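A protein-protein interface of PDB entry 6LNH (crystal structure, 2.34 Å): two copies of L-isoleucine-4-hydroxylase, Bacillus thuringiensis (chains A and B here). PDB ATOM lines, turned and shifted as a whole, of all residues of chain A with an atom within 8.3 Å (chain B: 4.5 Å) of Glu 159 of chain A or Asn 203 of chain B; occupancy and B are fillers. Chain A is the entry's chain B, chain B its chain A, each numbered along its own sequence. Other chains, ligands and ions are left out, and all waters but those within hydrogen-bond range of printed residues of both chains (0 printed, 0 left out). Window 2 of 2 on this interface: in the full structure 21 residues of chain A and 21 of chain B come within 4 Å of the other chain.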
ATOM      1  N   ALA A 156     -20.126  -2.460 -21.860  1.00  0.00           N
ATOM      2  CA  ALA A 156     -19.133  -1.659 -21.115  1.00  0.00           C
ATOM      3  C   ALA A 156     -17.884  -1.480 -21.978  1.00  0.00           C
ATOM      4  O   ALA A 156     -17.500  -2.426 -22.678  1.00  0.00           O
ATOM      5  CB  ALA A 156     -18.810  -2.320 -19.800  1.00  0.00           C
ATOM      6  N   THR A 157     -17.294  -0.290 -21.916  1.00  0.00           N
ATOM      7  CA  THR A 157     -16.068   0.043 -22.681  1.00  0.00           C
ATOM      8  C   THR A 157     -15.106   0.766 -21.730  1.00  0.00           C
ATOM      9  O   THR A 157     -15.577   1.308 -20.718  1.00  0.00           O
ATOM     10  CB  THR A 157     -16.439   0.769 -23.981  1.00  0.00           C
ATOM     11  OG1 THR A 157     -15.967  -0.014 -25.077  1.00  0.00           O
ATOM     12  CG2 THR A 157     -15.894   2.174 -24.084  1.00  0.00           C
ATOM     13  N   LYS A 158     -13.808   0.768 -22.037  1.00  0.00           N
ATOM     14  CA  LYS A 158     -12.806   1.432 -21.160  1.00  0.00           C
ATOM     15  C   LYS A 158     -13.206   2.890 -20.896  1.00  0.00           C
ATOM     16  O   LYS A 158     -13.142   3.308 -19.731  1.00  0.00           O
ATOM     17  CB  LYS A 158     -11.410   1.347 -21.784  1.00  0.00           C
ATOM     18  CG  LYS A 158     -10.252   1.501 -20.809  1.00  0.00           C
ATOM     19  CD  LYS A 158      -8.964   1.935 -21.473  1.00  0.00           C
ATOM     20  CE  LYS A 158      -8.232   0.799 -22.155  1.00  0.00           C
ATOM     21  NZ  LYS A 158      -8.036   1.068 -23.599  1.00  0.00           N
ATOM     22  N   GLU A 159     -13.603   3.627 -21.936  1.00  0.00           N
ATOM     23  CA  GLU A 159     -13.974   5.058 -21.788  1.00  0.00           C
ATOM     24  C   GLU A 159     -15.470   5.219 -21.489  1.00  0.00           C
ATOM     25  O   GLU A 159     -15.878   6.354 -21.197  1.00  0.00           O
ATOM     26  CB  GLU A 159     -13.606   5.818 -23.061  1.00  0.00           C
ATOM     27  CG  GLU A 159     -12.192   5.544 -23.538  1.00  0.00           C
ATOM     28  CD  GLU A 159     -11.969   4.164 -24.134  1.00  0.00           C
ATOM     29  OE1 GLU A 159     -10.867   3.921 -24.659  1.00  0.00           O
ATOM     30  OE2 GLU A 159     -12.895   3.339 -24.069  1.00  0.00           O
ATOM     31  N   ARG A 160     -16.251   4.138 -21.528  1.00  0.00           N
ATOM     32  CA  ARG A 160     -17.715   4.273 -21.302  1.00  0.00           C
ATOM     33  C   ARG A 160     -18.273   3.109 -20.475  1.00  0.00           C
ATOM     34  O   ARG A 160     -18.731   2.127 -21.078  1.00  0.00           O
ATOM     35  CB  ARG A 160     -18.444   4.344 -22.647  1.00  0.00           C
ATOM     36  CG  ARG A 160     -19.049   5.704 -22.959  1.00  0.00           C
ATOM     37  CD  ARG A 160     -20.447   5.585 -23.532  1.00  0.00           C
ATOM     38  NE  ARG A 160     -20.454   4.912 -24.822  1.00  0.00           N
ATOM     39  CZ  ARG A 160     -19.669   5.236 -25.842  1.00  0.00           C
ATOM     40  NH1 ARG A 160     -19.748   4.564 -26.978  1.00  0.00           N
ATOM     41  NH2 ARG A 160     -18.809   6.231 -25.723  1.00  0.00           N
ATOM     42  N   PRO A 161     -18.279   3.181 -19.126  1.00  0.00           N
ATOM     43  CA  PRO A 161     -18.864   2.121 -18.305  1.00  0.00           C
ATOM     44  C   PRO A 161     -20.396   2.160 -18.421  1.00  0.00           C
ATOM     45  O   PRO A 161     -20.935   3.211 -18.677  1.00  0.00           O
ATOM     46  CB  PRO A 161     -18.399   2.460 -16.885  1.00  0.00           C
ATOM     47  CG  PRO A 161     -18.144   3.947 -16.919  1.00  0.00           C
ATOM     48  CD  PRO A 161     -17.688   4.249 -18.330  1.00  0.00           C
ATOM     49  N   SER A 162     -21.051   1.016 -18.215  1.00  0.00           N
ATOM     50  CA  SER A 162     -22.528   0.925 -18.351  1.00  0.00           C
ATOM     51  C   SER A 162     -23.220   1.097 -16.995  1.00  0.00           C
ATOM     52  O   SER A 162     -22.777   0.462 -16.028  1.00  0.00           O
ATOM     53  CB  SER A 162     -22.912  -0.377 -18.993  1.00  0.00           C
ATOM     54  OG  SER A 162     -24.312  -0.573 -18.932  1.00  0.00           O
ATOM     55  N   PHE A 163     -24.268   1.926 -16.939  1.00  0.00           N
ATOM     56  CA  PHE A 163     -25.008   2.119 -15.706  1.00  0.00           C
ATOM     57  C   PHE A 163     -26.502   2.188 -15.932  1.00  0.00           C
ATOM     58  O   PHE A 163     -26.936   2.465 -17.002  1.00  0.00           O
ATOM     59  CB  PHE A 163     -24.524   3.386 -14.992  1.00  0.00           C
ATOM     60  CG  PHE A 163     -24.491   4.646 -15.789  1.00  0.00           C
ATOM     61  CD1 PHE A 163     -23.498   4.861 -16.728  1.00  0.00           C
ATOM     62  CD2 PHE A 163     -25.464   5.615 -15.604  1.00  0.00           C
ATOM     63  CE1 PHE A 163     -23.477   6.034 -17.490  1.00  0.00           C
ATOM     64  CE2 PHE A 163     -25.444   6.779 -16.365  1.00  0.00           C
ATOM     65  CZ  PHE A 163     -24.457   6.992 -17.299  1.00  0.00           C
ATOM     66  N   ILE A 167     -29.609   4.622 -10.906  1.00  0.00           N
ATOM     67  CA  ILE A 167     -28.171   4.231 -10.819  1.00  0.00           C
ATOM     68  C   ILE A 167     -27.848   3.555  -9.479  1.00  0.00           C
ATOM     69  O   ILE A 167     -26.978   2.674  -9.476  1.00  0.00           O
ATOM     70  CB  ILE A 167     -27.289   5.465 -11.104  1.00  0.00           C
ATOM     71  CG1 ILE A 167     -25.824   5.102 -11.343  1.00  0.00           C
ATOM     72  CG2 ILE A 167     -27.447   6.526 -10.025  1.00  0.00           C
ATOM     73  CD1 ILE A 167     -25.010   6.243 -11.897  1.00  0.00           C
ATOM     74  N   PRO A 227     -22.221  -0.714 -11.347  1.00  0.00           N
ATOM     75  CA  PRO A 227     -21.893  -0.442 -12.753  1.00  0.00           C
ATOM     76  C   PRO A 227     -20.974  -1.503 -13.343  1.00  0.00           C
ATOM     77  O   PRO A 227     -20.237  -2.187 -12.631  1.00  0.00           O
ATOM     78  CB  PRO A 227     -21.207   0.927 -12.700  1.00  0.00           C
ATOM     79  CG  PRO A 227     -21.767   1.561 -11.473  1.00  0.00           C
ATOM     80  CD  PRO A 227     -21.906   0.440 -10.488  1.00  0.00           C
ATOM     81  N   GLY A 229     -17.832  -2.294 -15.887  1.00  0.00           N
ATOM     82  CA  GLY A 229     -16.661  -1.658 -16.446  1.00  0.00           C
ATOM     83  C   GLY A 229     -15.740  -2.672 -17.121  1.00  0.00           C
ATOM     84  O   GLY A 229     -16.003  -3.874 -17.107  1.00  0.00           O
ATOM     85  N   THR A 230     -14.673  -2.139 -17.708  1.00  0.00           N
ATOM     86  CA  THR A 230     -13.597  -2.973 -18.236  1.00  0.00           C
ATOM     87  C   THR A 230     -12.307  -2.163 -18.285  1.00  0.00           C
ATOM     88  O   THR A 230     -12.328  -0.966 -18.578  1.00  0.00           O
ATOM     89  CB  THR A 230     -13.943  -3.514 -19.635  1.00  0.00           C
ATOM     90  OG1 THR A 230     -12.994  -4.517 -20.017  1.00  0.00           O
ATOM     91  CG2 THR A 230     -13.943  -2.401 -20.678  1.00  0.00           C
ATOM     92  N   GLU A 231     -11.204  -2.799 -17.903  1.00  0.00           N
ATOM     93  CA  GLU A 231      -9.855  -2.305 -18.204  1.00  0.00           C
ATOM     94  C   GLU A 231      -9.188  -3.090 -19.332  1.00  0.00           C
ATOM     95  O   GLU A 231      -8.077  -3.619 -19.203  1.00  0.00           O
ATOM     96  CB  GLU A 231      -9.003  -2.286 -16.947  1.00  0.00           C
ATOM     97  CG  GLU A 231      -9.659  -1.494 -15.842  1.00  0.00           C
ATOM     98  CD  GLU A 231      -9.106  -1.825 -14.482  1.00  0.00           C
ATOM     99  OE1 GLU A 231      -9.166  -0.952 -13.591  1.00  0.00           O
ATOM    100  OE2 GLU A 231      -8.593  -2.948 -14.309  1.00  0.00           O
ATOM    101  N   CYS A 232      -9.920  -3.258 -20.427  1.00  0.00           N
ATOM    102  CA  CYS A 232      -9.414  -3.940 -21.605  1.00  0.00           C
ATOM    103  C   CYS A 232      -9.745  -3.090 -22.822  1.00  0.00           C
ATOM    104  O   CYS A 232     -10.605  -2.210 -22.767  1.00  0.00           O
ATOM    105  CB  CYS A 232     -10.001  -5.352 -21.726  1.00  0.00           C
ATOM    106  SG  CYS A 232      -9.546  -6.442 -20.346  1.00  0.00           S
ATOM    107  N   SER A 233      -9.063  -3.362 -23.932  1.00  0.00           N
ATOM    108  CA  SER A 233      -9.299  -2.583 -25.141  1.00  0.00           C
ATOM    109  C   SER A 233     -10.528  -3.059 -25.898  1.00  0.00           C
ATOM    110  O   SER A 233     -10.920  -2.419 -26.880  1.00  0.00           O
ATOM    111  CB  SER A 233      -8.077  -2.631 -26.060  1.00  0.00           C
ATOM    112  OG  SER A 233      -6.875  -2.479 -25.323  1.00  0.00           O
ATOM    113  N   THR A 234     -11.108  -4.178 -25.463  1.00  0.00           N
ATOM    114  CA  THR A 234     -12.293  -4.756 -26.149  1.00  0.00           C
ATOM    115  C   THR A 234     -13.572  -4.381 -25.394  1.00  0.00           C
ATOM    116  O   THR A 234     -13.463  -3.862 -24.275  1.00  0.00           O
ATOM    117  CB  THR A 234     -12.147  -6.274 -26.296  1.00  0.00           C
ATOM    118  OG1 THR A 234     -12.237  -6.848 -24.992  1.00  0.00           O
ATOM    119  CG2 THR A 234     -10.836  -6.674 -26.934  1.00  0.00           C
ATOM    120  N   ILE B 195     -15.921   7.083 -10.962  1.00  0.00           N
ATOM    121  CA  ILE B 195     -15.742   8.512 -11.199  1.00  0.00           C
ATOM    122  C   ILE B 195     -16.976   9.019 -11.930  1.00  0.00           C
ATOM    123  O   ILE B 195     -17.388   8.434 -12.938  1.00  0.00           O
ATOM    124  CB  ILE B 195     -14.462   8.806 -12.001  1.00  0.00           C
ATOM    125  CG1 ILE B 195     -13.250   8.165 -11.319  1.00  0.00           C
ATOM    126  CG2 ILE B 195     -14.260  10.307 -12.145  1.00  0.00           C
ATOM    127  CD1 ILE B 195     -12.848   8.840 -10.024  1.00  0.00           C
ATOM    128  N   ALA B 196     -17.559  10.109 -11.429  1.00  0.00           N
ATOM    129  CA  ALA B 196     -18.788  10.659 -11.988  1.00  0.00           C
ATOM    130  C   ALA B 196     -18.707  12.174 -12.107  1.00  0.00           C
ATOM    131  O   ALA B 196     -18.371  12.855 -11.135  1.00  0.00           O
ATOM    132  CB  ALA B 196     -19.986  10.276 -11.114  1.00  0.00           C
ATOM    133  N   ASN B 197     -19.010  12.699 -13.300  1.00  0.00           N
ATOM    134  CA  ASN B 197     -19.149  14.146 -13.446  1.00  0.00           C
ATOM    135  C   ASN B 197     -20.362  14.664 -12.681  1.00  0.00           C
ATOM    136  O   ASN B 197     -20.317  15.756 -12.102  1.00  0.00           O
ATOM    137  CB  ASN B 197     -19.264  14.531 -14.925  1.00  0.00           C
ATOM    138  CG  ASN B 197     -18.051  14.114 -15.744  1.00  0.00           C
ATOM    139  OD1 ASN B 197     -16.946  13.987 -15.219  1.00  0.00           O
ATOM    140  ND2 ASN B 197     -18.256  13.904 -17.040  1.00  0.00           N
ATOM    141  N   SER B 198     -21.457  13.901 -12.672  1.00  0.00           N
ATOM    142  CA  SER B 198     -22.669  14.249 -11.927  1.00  0.00           C
ATOM    143  C   SER B 198     -23.233  13.010 -11.238  1.00  0.00           C
ATOM    144  O   SER B 198     -22.828  11.890 -11.577  1.00  0.00           O
ATOM    145  CB  SER B 198     -23.725  14.867 -12.850  1.00  0.00           C
ATOM    146  OG  SER B 198     -24.239  13.916 -13.767  1.00  0.00           O
ATOM    147  N   GLU B 201     -24.483   9.985 -13.605  1.00  0.00           N
ATOM    148  CA  GLU B 201     -23.803   9.231 -14.612  1.00  0.00           C
ATOM    149  C   GLU B 201     -22.525   8.688 -14.023  1.00  0.00           C
ATOM    150  O   GLU B 201     -21.956   9.245 -13.084  1.00  0.00           O
ATOM    151  CB  GLU B 201     -23.548  10.103 -15.836  1.00  0.00           C
ATOM    152  CG  GLU B 201     -22.891  11.416 -15.489  1.00  0.00           C
ATOM    153  CD  GLU B 201     -22.338  12.132 -16.703  1.00  0.00           C
ATOM    154  OE1 GLU B 201     -22.426  11.576 -17.815  1.00  0.00           O
ATOM    155  OE2 GLU B 201     -21.804  13.250 -16.546  1.00  0.00           O
ATOM    156  N   ILE B 202     -22.113   7.557 -14.564  1.00  0.00           N
ATOM    157  CA  ILE B 202     -20.821   6.973 -14.260  1.00  0.00           C
ATOM    158  C   ILE B 202     -19.953   7.188 -15.488  1.00  0.00           C
ATOM    159  O   ILE B 202     -20.320   6.769 -16.593  1.00  0.00           O
ATOM    160  CB  ILE B 202     -20.942   5.487 -13.906  1.00  0.00           C
ATOM    161  CG1 ILE B 202     -21.895   5.311 -12.718  1.00  0.00           C
ATOM    162  CG2 ILE B 202     -19.582   4.921 -13.614  1.00  0.00           C
ATOM    163  CD1 ILE B 202     -21.407   5.955 -11.433  1.00  0.00           C
ATOM    164  N   ASN B 203     -18.819   7.860 -15.304  1.00  0.00           N
ATOM    165  CA  ASN B 203     -17.952   8.196 -16.425  1.00  0.00           C
ATOM    166  C   ASN B 203     -16.692   7.354 -16.501  1.00  0.00           C
ATOM    167  O   ASN B 203     -16.179   7.135 -17.598  1.00  0.00           O
ATOM    168  CB  ASN B 203     -17.572   9.679 -16.369  1.00  0.00           C
ATOM    169  CG  ASN B 203     -18.785  10.571 -16.202  1.00  0.00           C
ATOM    170  OD1 ASN B 203     -18.874  11.357 -15.262  1.00  0.00           O
ATOM    171  ND2 ASN B 203     -19.745  10.432 -17.111  1.00  0.00           N
ATOM    172  N   GLN B 204     -16.185   6.863 -15.377  1.00  0.00           N
ATOM    173  CA  GLN B 204     -14.975   6.057 -15.407  1.00  0.00           C
ATOM    174  C   GLN B 204     -15.027   5.061 -14.261  1.00  0.00           C
ATOM    175  O   GLN B 204     -15.480   5.380 -13.160  1.00  0.00           O
ATOM    176  CB  GLN B 204     -13.702   6.910 -15.331  1.00  0.00           C
ATOM    177  CG  GLN B 204     -12.425   6.147 -15.697  1.00  0.00           C
ATOM    178  CD  GLN B 204     -12.090   6.214 -17.179  1.00  0.00           C
ATOM    179  OE1 GLN B 204     -12.981   6.312 -18.024  1.00  0.00           O
ATOM    180  NE2 GLN B 204     -10.799   6.158 -17.502  1.00  0.00           N
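The backbone carbonyl oxygen of Ile 195 of chain B is in hydrogen-bond range of the backbone NH of Asn 203 of chain B (2.8 Å). N of Ile 195 of chain B sits at hydrogen-bond distance from O of Gln 204 of chain B, at 2.8 Å. The side-chain amide oxygen of Asn 203 of chain B lies close to the side-chain amide nitrogen of Asn 197 of chain B, at 3.2 Å. The side-chain amide nitrogen (ND2) of Asn 203 of chain B lies within hydrogen-bond range of the side-chain carboxylate (OE1) of Glu 201 of chain B.
OE1 of Gln 204 of chain B lies close to O of Lys 158 of chain A (3.5 Å).
Of the 8 printed residues of chain B, 4 touch a printed residue of chain A. Printed residues of chain B that touch a printed residue of chain A: Glu 201, Ile 202, Asn 203 and Gln 204. Of the 16 printed residues of chain A, 6 touch a printed residue of chain B. Hydrophobic or aromatic side chains of chain A within 4 Å of the printed part of chain B: Pro 161, Phe 163, Ile 167 and Pro 227. Among the printed residues, no Asp or Glu carboxylate lies within 4 Å of a Lys or Arg side-chain nitrogen of the other chain.
No position is printed for both chains. Of the 9 pairs that touch across the chains among the printed residues, none has its exchanged pair printed and touching as well.
Printed residues of chain B within 4 Å of Lys 158 of chain A: Gln 204. Of chain B, only Asn 203 comes within 4 Å of Glu 159 of chain A. Printed residues of chain B within 4 Å of Pro 227 of chain A: Ile 202 (3.95 Å). Glu 231 of chain A touches none of the printed residues of chain B. Thr 234 of chain A touches none of the printed residues of chain B. Printed residues of chain A within 4 Å of Glu 201 of chain B: Phe 163 (3.4 Å). Printed residues of chain A within 4 Å of Ile 202 of chain B: Pro 161, Phe 163, Ile 167 and Pro 227. Printed residues of chain A within 4 Å of Asn 203 of chain B: Glu 159 (3.7 Å) and Pro 161 (3.3 Å). Printed residues of chain A within 4 Å of Gln 204 of chain B: Lys 158 and Pro 161. The nearest residue of chain A that does not touch Asn 203 of chain B is Arg 160 of chain A (4.9 Å). The nearest printed residue of chain B that does not touch Pro 227 of chain A is Gln 204 of chain B (7.3 Å).
Glu 159 of chain A touches Asn 203 of chain B. CG of Pro 161 of chain A touches O of Ile 202 of chain B, at 3.6 Å. Pro 161 of chain A touches Asn 203 of chain B. Pro 161 of chain A touches Gln 204 of chain B. Phe 163 of chain A touches Glu 201 of chain B (CE2 to CA, 3.4 Å). Ile 202 of chain B touches Phe 163 of chain A. Ile 202 of chain B touches Ile 167 of chain A. Ile 202 of chain B touches Pro 227 of chain A.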
